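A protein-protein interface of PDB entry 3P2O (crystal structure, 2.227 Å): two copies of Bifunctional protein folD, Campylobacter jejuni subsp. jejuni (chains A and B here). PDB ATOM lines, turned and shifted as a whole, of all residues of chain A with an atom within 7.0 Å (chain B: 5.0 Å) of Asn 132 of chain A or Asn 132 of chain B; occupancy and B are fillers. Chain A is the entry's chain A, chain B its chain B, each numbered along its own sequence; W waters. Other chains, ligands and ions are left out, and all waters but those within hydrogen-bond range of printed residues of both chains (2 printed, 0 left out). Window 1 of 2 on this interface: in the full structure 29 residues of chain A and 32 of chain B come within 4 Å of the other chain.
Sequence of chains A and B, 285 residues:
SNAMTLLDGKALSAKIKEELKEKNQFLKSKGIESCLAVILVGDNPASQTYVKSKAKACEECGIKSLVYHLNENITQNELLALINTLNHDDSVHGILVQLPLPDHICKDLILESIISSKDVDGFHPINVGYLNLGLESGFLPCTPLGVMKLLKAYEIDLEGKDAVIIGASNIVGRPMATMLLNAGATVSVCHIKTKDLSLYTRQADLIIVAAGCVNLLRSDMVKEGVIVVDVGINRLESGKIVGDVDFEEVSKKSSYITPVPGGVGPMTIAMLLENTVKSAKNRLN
Among the printed residues, no Asp or Glu carboxylate lies within 4 Å of a Lys or Arg side-chain nitrogen of the other chain.
ND2 of Asn 132 of chain A lies close to ND2 of Asn 132 of chain B, 2.7 Å away.
OD1 of Asn 170 of chain B sits close to O of Asn 132 of chain A, 3.3 Å away.
O of Asn 132 of chain A lies within hydrogen-bond range of NH1 of Arg 174 of chain B (3.1 Å).
O of Leu 133 of chain A lies within hydrogen-bond range of ND2 of Asn 170 of chain B.
O of Asn 132 of chain B lies close to OD1 of Asn 170 of chain A, at 3.3 Å.
NH1 of Arg 174 of chain A is in hydrogen-bond range of O of Asn 132 of chain B, at 3.3 Å.
OD1 of Asn 182 of chain A sits at hydrogen-bond distance from NH1 of Arg 174 of chain B (2.8 Å).
Asn 132 of chain A touches just these residues of chain B: Val 128 (3.7 Å), Asn 132 (2.7 Å), Asn 170 (3.3 Å) and Arg 174 (3.1 Å).
Of chain A, only Val 128 (3.8 Å), Asn 132 (2.7 Å), Asn 170 (3.3 Å) and Arg 174 (3.3 Å) come within 4 Å of Asn 132 of chain B.
Of the printed residues of chain A, Thr 178 of chain B touches Arg 174.
Printed residues of chain A within 4 Å of Gly 129 of chain B: Val 128 (3.9 Å) and Gly 129 (3.7 Å).
Of the printed residues of chain B, Asn 182 of chain A touches Arg 174 (2.8 Å).
Leu 135 of chain A touches none of the printed residues of chain B.
The nearest residue of chain B that does not touch Asn 132 of chain A is Thr 178 of chain B (4.2 Å).
The nearest residue of chain A that does not touch Asn 132 of chain B is Thr 178 of chain A (4.6 Å).
Val 128 of chain A touches Gly 129 of chain B.
Val 128 of chain A touches Asn 132 of chain B.
Val 128 of chain A touches Leu 133 of chain B (CG2 to CD2, 3.97 Å).
Gly 129 of chain A touches Val 128 of chain B.
Gly 129 of chain B touches Gly 129 of chain A.
Asn 132 of chain A touches Val 128 of chain B (CB to CG1, 3.7 Å).
Val 128 of chain B touches Leu 133 of chain A.
Asn 170 of chain A touches Leu 133 of chain B (ND2 to O, 3.5 Å).
Arg 174 of chain A touches Thr 178 of chain B (NH1 to CG2, 3.8 Å).
Arg 174 of chain B touches Leu 181 of chain A.
Val 128 of chain A touches Gly 129 of chain B, and with the chains exchanged Gly 129 of chain A touches Val 128 of chain B.
Val 128 of chain A touches Leu 133 of chain B, and with the chains exchanged Leu 133 of chain A touches Val 128 of chain B.
Asn 132 of chain A touches Asn 170 of chain B, and with the chains exchanged Asn 170 of chain A touches Asn 132 of chain B.
Leu 133 of chain A touches Asn 170 of chain B, and with the chains exchanged Asn 170 of chain A touches Leu 133 of chain B.
10 positions are printed for both chains.
Water W2 bridges the side-chain amide oxygen (OD1) of Asn 170 of chain A and the side-chain amide oxygen (OD1) of Asn 132 of chain B.
Water W1 lies within hydrogen-bond range of the side-chain amide oxygen of Asn 132 of chain A and the side-chain amide oxygen of Asn 170 of chain B.
The backbone carbonyl oxygen of Leu 131 of chain A lies within hydrogen-bond range of the side-chain amide nitrogen of Asn 182 of chain A.
O of Ala 168 of chain A sits at hydrogen-bond distance from NE of Arg 174 of chain A, 2.9 Å away.
The backbone carbonyl oxygen of Ser 169 of chain A is in hydrogen-bond range of the backbone NH of Arg 174 of chain A (2.9 Å).
O of Arg 174 of chain A is in hydrogen-bond range of OG1 of Thr 178 of chain A (3.0 Å).
O of Thr 178 of chain A sits close to OD1 of Asn 182 of chain A.
The side-chain hydroxyl of Thr 178 of chain B lies within hydrogen-bond range of the backbone carbonyl oxygen of Arg 174 of chain B (3.0 Å).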
ATOM      1  N   ASN A 127     -15.212  -2.119  21.922  1.00  0.00           N
ATOM      2  CA  ASN A 127     -16.208  -3.187  21.846  1.00  0.00           C
ATOM      3  C   ASN A 127     -17.624  -2.653  22.022  1.00  0.00           C
ATOM      4  O   ASN A 127     -18.559  -3.132  21.384  1.00  0.00           O
ATOM      5  CB  ASN A 127     -15.913  -4.291  22.862  1.00  0.00           C
ATOM      6  CG  ASN A 127     -14.891  -5.283  22.346  1.00  0.00           C
ATOM      7  OD1 ASN A 127     -14.859  -5.581  21.151  1.00  0.00           O
ATOM      8  ND2 ASN A 127     -14.061  -5.810  23.244  1.00  0.00           N
ATOM      9  N   VAL A 128     -17.775  -1.648  22.869  1.00  0.00           N
ATOM     10  CA  VAL A 128     -19.068  -0.981  23.006  1.00  0.00           C
ATOM     11  C   VAL A 128     -19.422  -0.293  21.675  1.00  0.00           C
ATOM     12  O   VAL A 128     -20.585  -0.251  21.278  1.00  0.00           O
ATOM     13  CB  VAL A 128     -19.032   0.045  24.132  1.00  0.00           C
ATOM     14  CG1 VAL A 128     -20.270   0.954  24.076  1.00  0.00           C
ATOM     15  CG2 VAL A 128     -18.886  -0.672  25.512  1.00  0.00           C
ATOM     16  N   GLY A 129     -18.406   0.211  20.970  1.00  0.00           N
ATOM     17  CA  GLY A 129     -18.649   0.881  19.704  1.00  0.00           C
ATOM     18  C   GLY A 129     -19.068  -0.071  18.601  1.00  0.00           C
ATOM     19  O   GLY A 129     -20.003   0.216  17.847  1.00  0.00           O
ATOM     20  N   TYR A 130     -18.388  -1.211  18.496  1.00  0.00           N
ATOM     21  CA  TYR A 130     -18.739  -2.209  17.485  1.00  0.00           C
ATOM     22  C   TYR A 130     -20.216  -2.596  17.589  1.00  0.00           C
ATOM     23  O   TYR A 130     -20.919  -2.690  16.584  1.00  0.00           O
ATOM     24  CB  TYR A 130     -17.874  -3.474  17.625  1.00  0.00           C
ATOM     25  CG  TYR A 130     -16.396  -3.322  17.222  1.00  0.00           C
ATOM     26  CD1 TYR A 130     -16.013  -2.515  16.166  1.00  0.00           C
ATOM     27  CD2 TYR A 130     -15.405  -4.011  17.911  1.00  0.00           C
ATOM     28  CE1 TYR A 130     -14.675  -2.386  15.794  1.00  0.00           C
ATOM     29  CE2 TYR A 130     -14.091  -3.894  17.581  1.00  0.00           C
ATOM     30  CZ  TYR A 130     -13.719  -3.076  16.515  1.00  0.00           C
ATOM     31  OH  TYR A 130     -12.394  -2.987  16.186  1.00  0.00           O
ATOM     32  N   LEU A 131     -20.670  -2.852  18.813  1.00  0.00           N
ATOM     33  CA  LEU A 131     -22.052  -3.227  19.060  1.00  0.00           C
ATOM     34  C   LEU A 131     -23.038  -2.158  18.561  1.00  0.00           C
ATOM     35  O   LEU A 131     -23.952  -2.440  17.796  1.00  0.00           O
ATOM     36  CB  LEU A 131     -22.249  -3.485  20.562  1.00  0.00           C
ATOM     37  CG  LEU A 131     -23.683  -3.873  20.905  1.00  0.00           C
ATOM     38  CD1 LEU A 131     -24.090  -4.976  19.971  1.00  0.00           C
ATOM     39  CD2 LEU A 131     -23.744  -4.352  22.348  1.00  0.00           C
ATOM     40  N   ASN A 132     -22.816  -0.926  18.985  1.00  0.00           N
ATOM     41  CA  ASN A 132     -23.655   0.204  18.623  1.00  0.00           C
ATOM     42  C   ASN A 132     -23.711   0.442  17.123  1.00  0.00           C
ATOM     43  O   ASN A 132     -24.670   1.006  16.618  1.00  0.00           O
ATOM     44  CB  ASN A 132     -23.167   1.444  19.369  1.00  0.00           C
ATOM     45  CG  ASN A 132     -24.200   2.569  19.406  1.00  0.00           C
ATOM     46  OD1 ASN A 132     -24.385   3.289  18.430  1.00  0.00           O
ATOM     47  ND2 ASN A 132     -24.852   2.737  20.547  1.00  0.00           N
ATOM     48  N   LEU A 133     -22.693  -0.012  16.404  1.00  0.00           N
ATOM     49  CA  LEU A 133     -22.633   0.169  14.955  1.00  0.00           C
ATOM     50  C   LEU A 133     -23.341  -0.988  14.281  1.00  0.00           C
ATOM     51  O   LEU A 133     -23.505  -0.998  13.068  1.00  0.00           O
ATOM     52  CB  LEU A 133     -21.179   0.178  14.471  1.00  0.00           C
ATOM     53  CG  LEU A 133     -20.258   1.336  14.841  1.00  0.00           C
ATOM     54  CD1 LEU A 133     -18.809   1.030  14.428  1.00  0.00           C
ATOM     55  CD2 LEU A 133     -20.779   2.632  14.210  1.00  0.00           C
ATOM     56  N   GLY A 134     -23.706  -2.000  15.060  1.00  0.00           N
ATOM     57  CA  GLY A 134     -24.447  -3.111  14.498  1.00  0.00           C
ATOM     58  C   GLY A 134     -23.627  -4.348  14.186  1.00  0.00           C
ATOM     59  O   GLY A 134     -24.162  -5.330  13.664  1.00  0.00           O
ATOM     60  N   LEU A 135     -22.334  -4.304  14.511  1.00  0.00           N
ATOM     61  CA  LEU A 135     -21.435  -5.440  14.301  1.00  0.00           C
ATOM     62  C   LEU A 135     -21.509  -6.308  15.524  1.00  0.00           C
ATOM     63  O   LEU A 135     -21.296  -5.828  16.623  1.00  0.00           O
ATOM     64  CB  LEU A 135     -19.988  -4.969  14.149  1.00  0.00           C
ATOM     65  CG  LEU A 135     -19.880  -3.708  13.307  1.00  0.00           C
ATOM     66  CD1 LEU A 135     -18.449  -3.199  13.281  1.00  0.00           C
ATOM     67  CD2 LEU A 135     -20.385  -3.999  11.916  1.00  0.00           C
ATOM     68  N   ALA A 168     -31.011   1.663  32.297  1.00  0.00           N
ATOM     69  CA  ALA A 168     -30.150   2.135  31.211  1.00  0.00           C
ATOM     70  C   ALA A 168     -28.619   2.074  31.503  1.00  0.00           C
ATOM     71  O   ALA A 168     -27.845   2.944  31.052  1.00  0.00           O
ATOM     72  CB  ALA A 168     -30.559   3.563  30.783  1.00  0.00           C
ATOM     73  N   SER A 169     -28.179   1.055  32.237  1.00  0.00           N
ATOM     74  CA  SER A 169     -26.772   0.983  32.625  1.00  0.00           C
ATOM     75  C   SER A 169     -25.897   0.507  31.472  1.00  0.00           C
ATOM     76  O   SER A 169     -26.379  -0.033  30.465  1.00  0.00           O
ATOM     77  CB  SER A 169     -26.557   0.022  33.792  1.00  0.00           C
ATOM     78  OG  SER A 169     -26.572  -1.294  33.286  1.00  0.00           O
ATOM     79  N   ASN A 170     -24.596   0.650  31.663  1.00  0.00           N
ATOM     80  CA  ASN A 170     -23.634   0.172  30.664  1.00  0.00           C
ATOM     81  C   ASN A 170     -23.491  -1.335  30.713  1.00  0.00           C
ATOM     82  O   ASN A 170     -23.221  -1.975  29.695  1.00  0.00           O
ATOM     83  CB  ASN A 170     -22.287   0.898  30.821  1.00  0.00           C
ATOM     84  CG  ASN A 170     -22.380   2.355  30.416  1.00  0.00           C
ATOM     85  OD1 ASN A 170     -22.963   2.677  29.389  1.00  0.00           O
ATOM     86  ND2 ASN A 170     -21.814   3.243  31.218  1.00  0.00           N
ATOM     87  N   ARG A 174     -28.221  -0.449  28.298  1.00  0.00           N
ATOM     88  CA  ARG A 174     -27.854   0.117  26.998  1.00  0.00           C
ATOM     89  C   ARG A 174     -27.453  -0.924  25.967  1.00  0.00           C
ATOM     90  O   ARG A 174     -27.900  -0.837  24.830  1.00  0.00           O
ATOM     91  CB  ARG A 174     -26.797   1.201  27.138  1.00  0.00           C
ATOM     92  CG  ARG A 174     -27.289   2.394  27.909  1.00  0.00           C
ATOM     93  CD  ARG A 174     -26.138   3.268  28.236  1.00  0.00           C
ATOM     94  NE  ARG A 174     -26.505   4.471  28.966  1.00  0.00           N
ATOM     95  CZ  ARG A 174     -26.338   5.706  28.505  1.00  0.00           C
ATOM     96  NH1 ARG A 174     -25.848   5.907  27.287  1.00  0.00           N
ATOM     97  NH2 ARG A 174     -26.676   6.746  29.261  1.00  0.00           N
ATOM     98  N   PRO A 175     -26.604  -1.915  26.349  1.00  0.00           N
ATOM     99  CA  PRO A 175     -26.313  -2.935  25.336  1.00  0.00           C
ATOM    100  C   PRO A 175     -27.523  -3.801  25.012  1.00  0.00           C
ATOM    101  O   PRO A 175     -27.673  -4.222  23.859  1.00  0.00           O
ATOM    102  CB  PRO A 175     -25.207  -3.794  25.984  1.00  0.00           C
ATOM    103  CG  PRO A 175     -25.117  -3.348  27.421  1.00  0.00           C
ATOM    104  CD  PRO A 175     -25.593  -1.922  27.426  1.00  0.00           C
ATOM    105  N   THR A 178     -29.499  -1.987  22.422  1.00  0.00           N
ATOM    106  CA  THR A 178     -28.813  -1.964  21.147  1.00  0.00           C
ATOM    107  C   THR A 178     -29.014  -3.312  20.461  1.00  0.00           C
ATOM    108  O   THR A 178     -29.299  -3.377  19.259  1.00  0.00           O
ATOM    109  CB  THR A 178     -27.297  -1.659  21.338  1.00  0.00           C
ATOM    110  OG1 THR A 178     -27.147  -0.370  21.931  1.00  0.00           O
ATOM    111  CG2 THR A 178     -26.561  -1.701  20.026  1.00  0.00           C
ATOM    112  N   LEU A 181     -32.505  -3.617  19.172  1.00  0.00           N
ATOM    113  CA  LEU A 181     -32.631  -2.732  18.018  1.00  0.00           C
ATOM    114  C   LEU A 181     -31.885  -3.305  16.807  1.00  0.00           C
ATOM    115  O   LEU A 181     -32.330  -3.160  15.660  1.00  0.00           O
ATOM    116  CB  LEU A 181     -32.094  -1.365  18.382  1.00  0.00           C
ATOM    117  CG  LEU A 181     -31.928  -0.416  17.213  1.00  0.00           C
ATOM    118  CD1 LEU A 181     -33.290  -0.204  16.559  1.00  0.00           C
ATOM    119  CD2 LEU A 181     -31.364   0.883  17.762  1.00  0.00           C
ATOM    120  N   ASN A 182     -30.748  -3.958  17.071  1.00  0.00           N
ATOM    121  CA  ASN A 182     -29.999  -4.661  16.023  1.00  0.00           C
ATOM    122  C   ASN A 182     -30.813  -5.802  15.428  1.00  0.00           C
ATOM    123  O   ASN A 182     -30.619  -6.172  14.267  1.00  0.00           O
ATOM    124  CB  ASN A 182     -28.680  -5.240  16.555  1.00  0.00           C
ATOM    125  CG  ASN A 182     -27.598  -4.194  16.715  1.00  0.00           C
ATOM    126  OD1 ASN A 182     -27.730  -3.058  16.244  1.00  0.00           O
ATOM    127  ND2 ASN A 182     -26.514  -4.571  17.394  1.00  0.00           N
ATOM    128  N   VAL B 128     -17.594   6.141  19.098  1.00  0.00           N
ATOM    129  CA  VAL B 128     -18.965   5.717  19.275  1.00  0.00           C
ATOM    130  C   VAL B 128     -19.078   5.111  20.695  1.00  0.00           C
ATOM    131  O   VAL B 128     -19.985   5.448  21.468  1.00  0.00           O
ATOM    132  CB  VAL B 128     -19.359   4.671  18.201  1.00  0.00           C
ATOM    133  CG1 VAL B 128     -20.741   4.068  18.500  1.00  0.00           C
ATOM    134  CG2 VAL B 128     -19.322   5.280  16.807  1.00  0.00           C
ATOM    135  N   GLY B 129     -18.113   4.259  21.040  1.00  0.00           N
ATOM    136  CA  GLY B 129     -18.075   3.621  22.344  1.00  0.00           C
ATOM    137  C   GLY B 129     -18.080   4.640  23.462  1.00  0.00           C
ATOM    138  O   GLY B 129     -18.867   4.544  24.401  1.00  0.00           O
ATOM    139  N   TYR B 130     -17.204   5.636  23.368  1.00  0.00           N
ATOM    140  CA  TYR B 130     -17.119   6.652  24.417  1.00  0.00           C
ATOM    141  C   TYR B 130     -18.489   7.279  24.687  1.00  0.00           C
ATOM    142  O   TYR B 130     -18.893   7.475  25.840  1.00  0.00           O
ATOM    143  CB  TYR B 130     -16.131   7.757  24.027  1.00  0.00           C
ATOM    144  CG  TYR B 130     -14.659   7.354  24.052  1.00  0.00           C
ATOM    145  CD1 TYR B 130     -14.180   6.449  24.993  1.00  0.00           C
ATOM    146  CD2 TYR B 130     -13.732   7.910  23.132  1.00  0.00           C
ATOM    147  CE1 TYR B 130     -12.816   6.086  25.036  1.00  0.00           C
ATOM    148  CE2 TYR B 130     -12.389   7.541  23.157  1.00  0.00           C
ATOM    149  CZ  TYR B 130     -11.938   6.635  24.109  1.00  0.00           C
ATOM    150  OH  TYR B 130     -10.618   6.276  24.150  1.00  0.00           O
ATOM    151  N   LEU B 131     -19.192   7.584  23.603  1.00  0.00           N
ATOM    152  CA  LEU B 131     -20.449   8.288  23.676  1.00  0.00           C
ATOM    153  C   LEU B 131     -21.493   7.393  24.313  1.00  0.00           C
ATOM    154  O   LEU B 131     -22.242   7.831  25.175  1.00  0.00           O
ATOM    155  CB  LEU B 131     -20.914   8.679  22.277  1.00  0.00           C
ATOM    156  CG  LEU B 131     -22.359   9.175  22.237  1.00  0.00           C
ATOM    157  CD1 LEU B 131     -22.465  10.479  23.020  1.00  0.00           C
ATOM    158  CD2 LEU B 131     -22.793   9.390  20.792  1.00  0.00           C
ATOM    159  N   ASN B 132     -21.529   6.136  23.883  1.00  0.00           N
ATOM    160  CA  ASN B 132     -22.507   5.199  24.393  1.00  0.00           C
ATOM    161  C   ASN B 132     -22.231   4.894  25.861  1.00  0.00           C
ATOM    162  O   ASN B 132     -23.078   4.341  26.561  1.00  0.00           O
ATOM    163  CB  ASN B 132     -22.581   3.925  23.557  1.00  0.00           C
ATOM    164  CG  ASN B 132     -23.837   3.097  23.878  1.00  0.00           C
ATOM    165  OD1 ASN B 132     -23.828   2.224  24.764  1.00  0.00           O
ATOM    166  ND2 ASN B 132     -24.935   3.407  23.187  1.00  0.00           N
ATOM    167  N   LEU B 133     -21.059   5.305  26.334  1.00  0.00           N
ATOM    168  CA  LEU B 133     -20.701   5.099  27.727  1.00  0.00           C
ATOM    169  C   LEU B 133     -21.027   6.333  28.547  1.00  0.00           C
ATOM    170  O   LEU B 133     -20.888   6.325  29.768  1.00  0.00           O
ATOM    171  CB  LEU B 133     -19.217   4.735  27.877  1.00  0.00           C
ATOM    172  CG  LEU B 133     -18.777   3.346  27.391  1.00  0.00           C
ATOM    173  CD1 LEU B 133     -17.265   3.153  27.559  1.00  0.00           C
ATOM    174  CD2 LEU B 133     -19.552   2.240  28.121  1.00  0.00           C
ATOM    175  N   GLY B 134     -21.472   7.391  27.883  1.00  0.00           N
ATOM    176  CA  GLY B 134     -21.803   8.621  28.584  1.00  0.00           C
ATOM    177  C   GLY B 134     -20.626   9.575  28.702  1.00  0.00           C
ATOM    178  O   GLY B 134     -20.699  10.584  29.415  1.00  0.00           O
ATOM    179  N   ASN B 170     -26.453   4.944  11.993  1.00  0.00           N
ATOM    180  CA  ASN B 170     -25.252   5.268  12.753  1.00  0.00           C
ATOM    181  C   ASN B 170     -24.870   6.745  12.604  1.00  0.00           C
ATOM    182  O   ASN B 170     -24.169   7.330  13.437  1.00  0.00           O
ATOM    183  CB  ASN B 170     -24.105   4.346  12.333  1.00  0.00           C
ATOM    184  CG  ASN B 170     -24.380   2.882  12.677  1.00  0.00           C
ATOM    185  OD1 ASN B 170     -24.901   2.576  13.752  1.00  0.00           O
ATOM    186  ND2 ASN B 170     -24.031   1.976  11.767  1.00  0.00           N
ATOM    187  N   ARG B 174     -28.973   6.578  16.018  1.00  0.00           N
ATOM    188  CA  ARG B 174     -28.387   5.931  17.193  1.00  0.00           C
ATOM    189  C   ARG B 174     -27.647   6.877  18.135  1.00  0.00           C
ATOM    190  O   ARG B 174     -27.971   6.926  19.338  1.00  0.00           O
ATOM    191  CB  ARG B 174     -27.565   4.716  16.782  1.00  0.00           C
ATOM    192  CG  ARG B 174     -28.421   3.641  16.099  1.00  0.00           C
ATOM    193  CD  ARG B 174     -27.592   2.495  15.596  1.00  0.00           C
ATOM    194  NE  ARG B 174     -28.371   1.425  14.988  1.00  0.00           N
ATOM    195  CZ  ARG B 174     -28.285   0.142  15.337  1.00  0.00           C
ATOM    196  NH1 ARG B 174     -27.459  -0.234  16.313  1.00  0.00           N
ATOM    197  NH2 ARG B 174     -29.036  -0.768  14.718  1.00  0.00           N
ATOM    198  N   THR B 178     -28.603   8.224  21.983  1.00  0.00           N
ATOM    199  CA  THR B 178     -27.653   8.101  23.092  1.00  0.00           C
ATOM    200  C   THR B 178     -27.423   9.445  23.757  1.00  0.00           C
ATOM    201  O   THR B 178     -27.342   9.557  24.981  1.00  0.00           O
ATOM    202  CB  THR B 178     -26.286   7.567  22.597  1.00  0.00           C
ATOM    203  OG1 THR B 178     -26.503   6.377  21.843  1.00  0.00           O
ATOM    204  CG2 THR B 178     -25.382   7.272  23.761  1.00  0.00           C
HETATM  205  O   HOH W   1     -23.807   3.918  15.872  1.00  0.00           O
HETATM  206  O   HOH W   2     -23.038   1.536  27.208  1.00  0.00           O
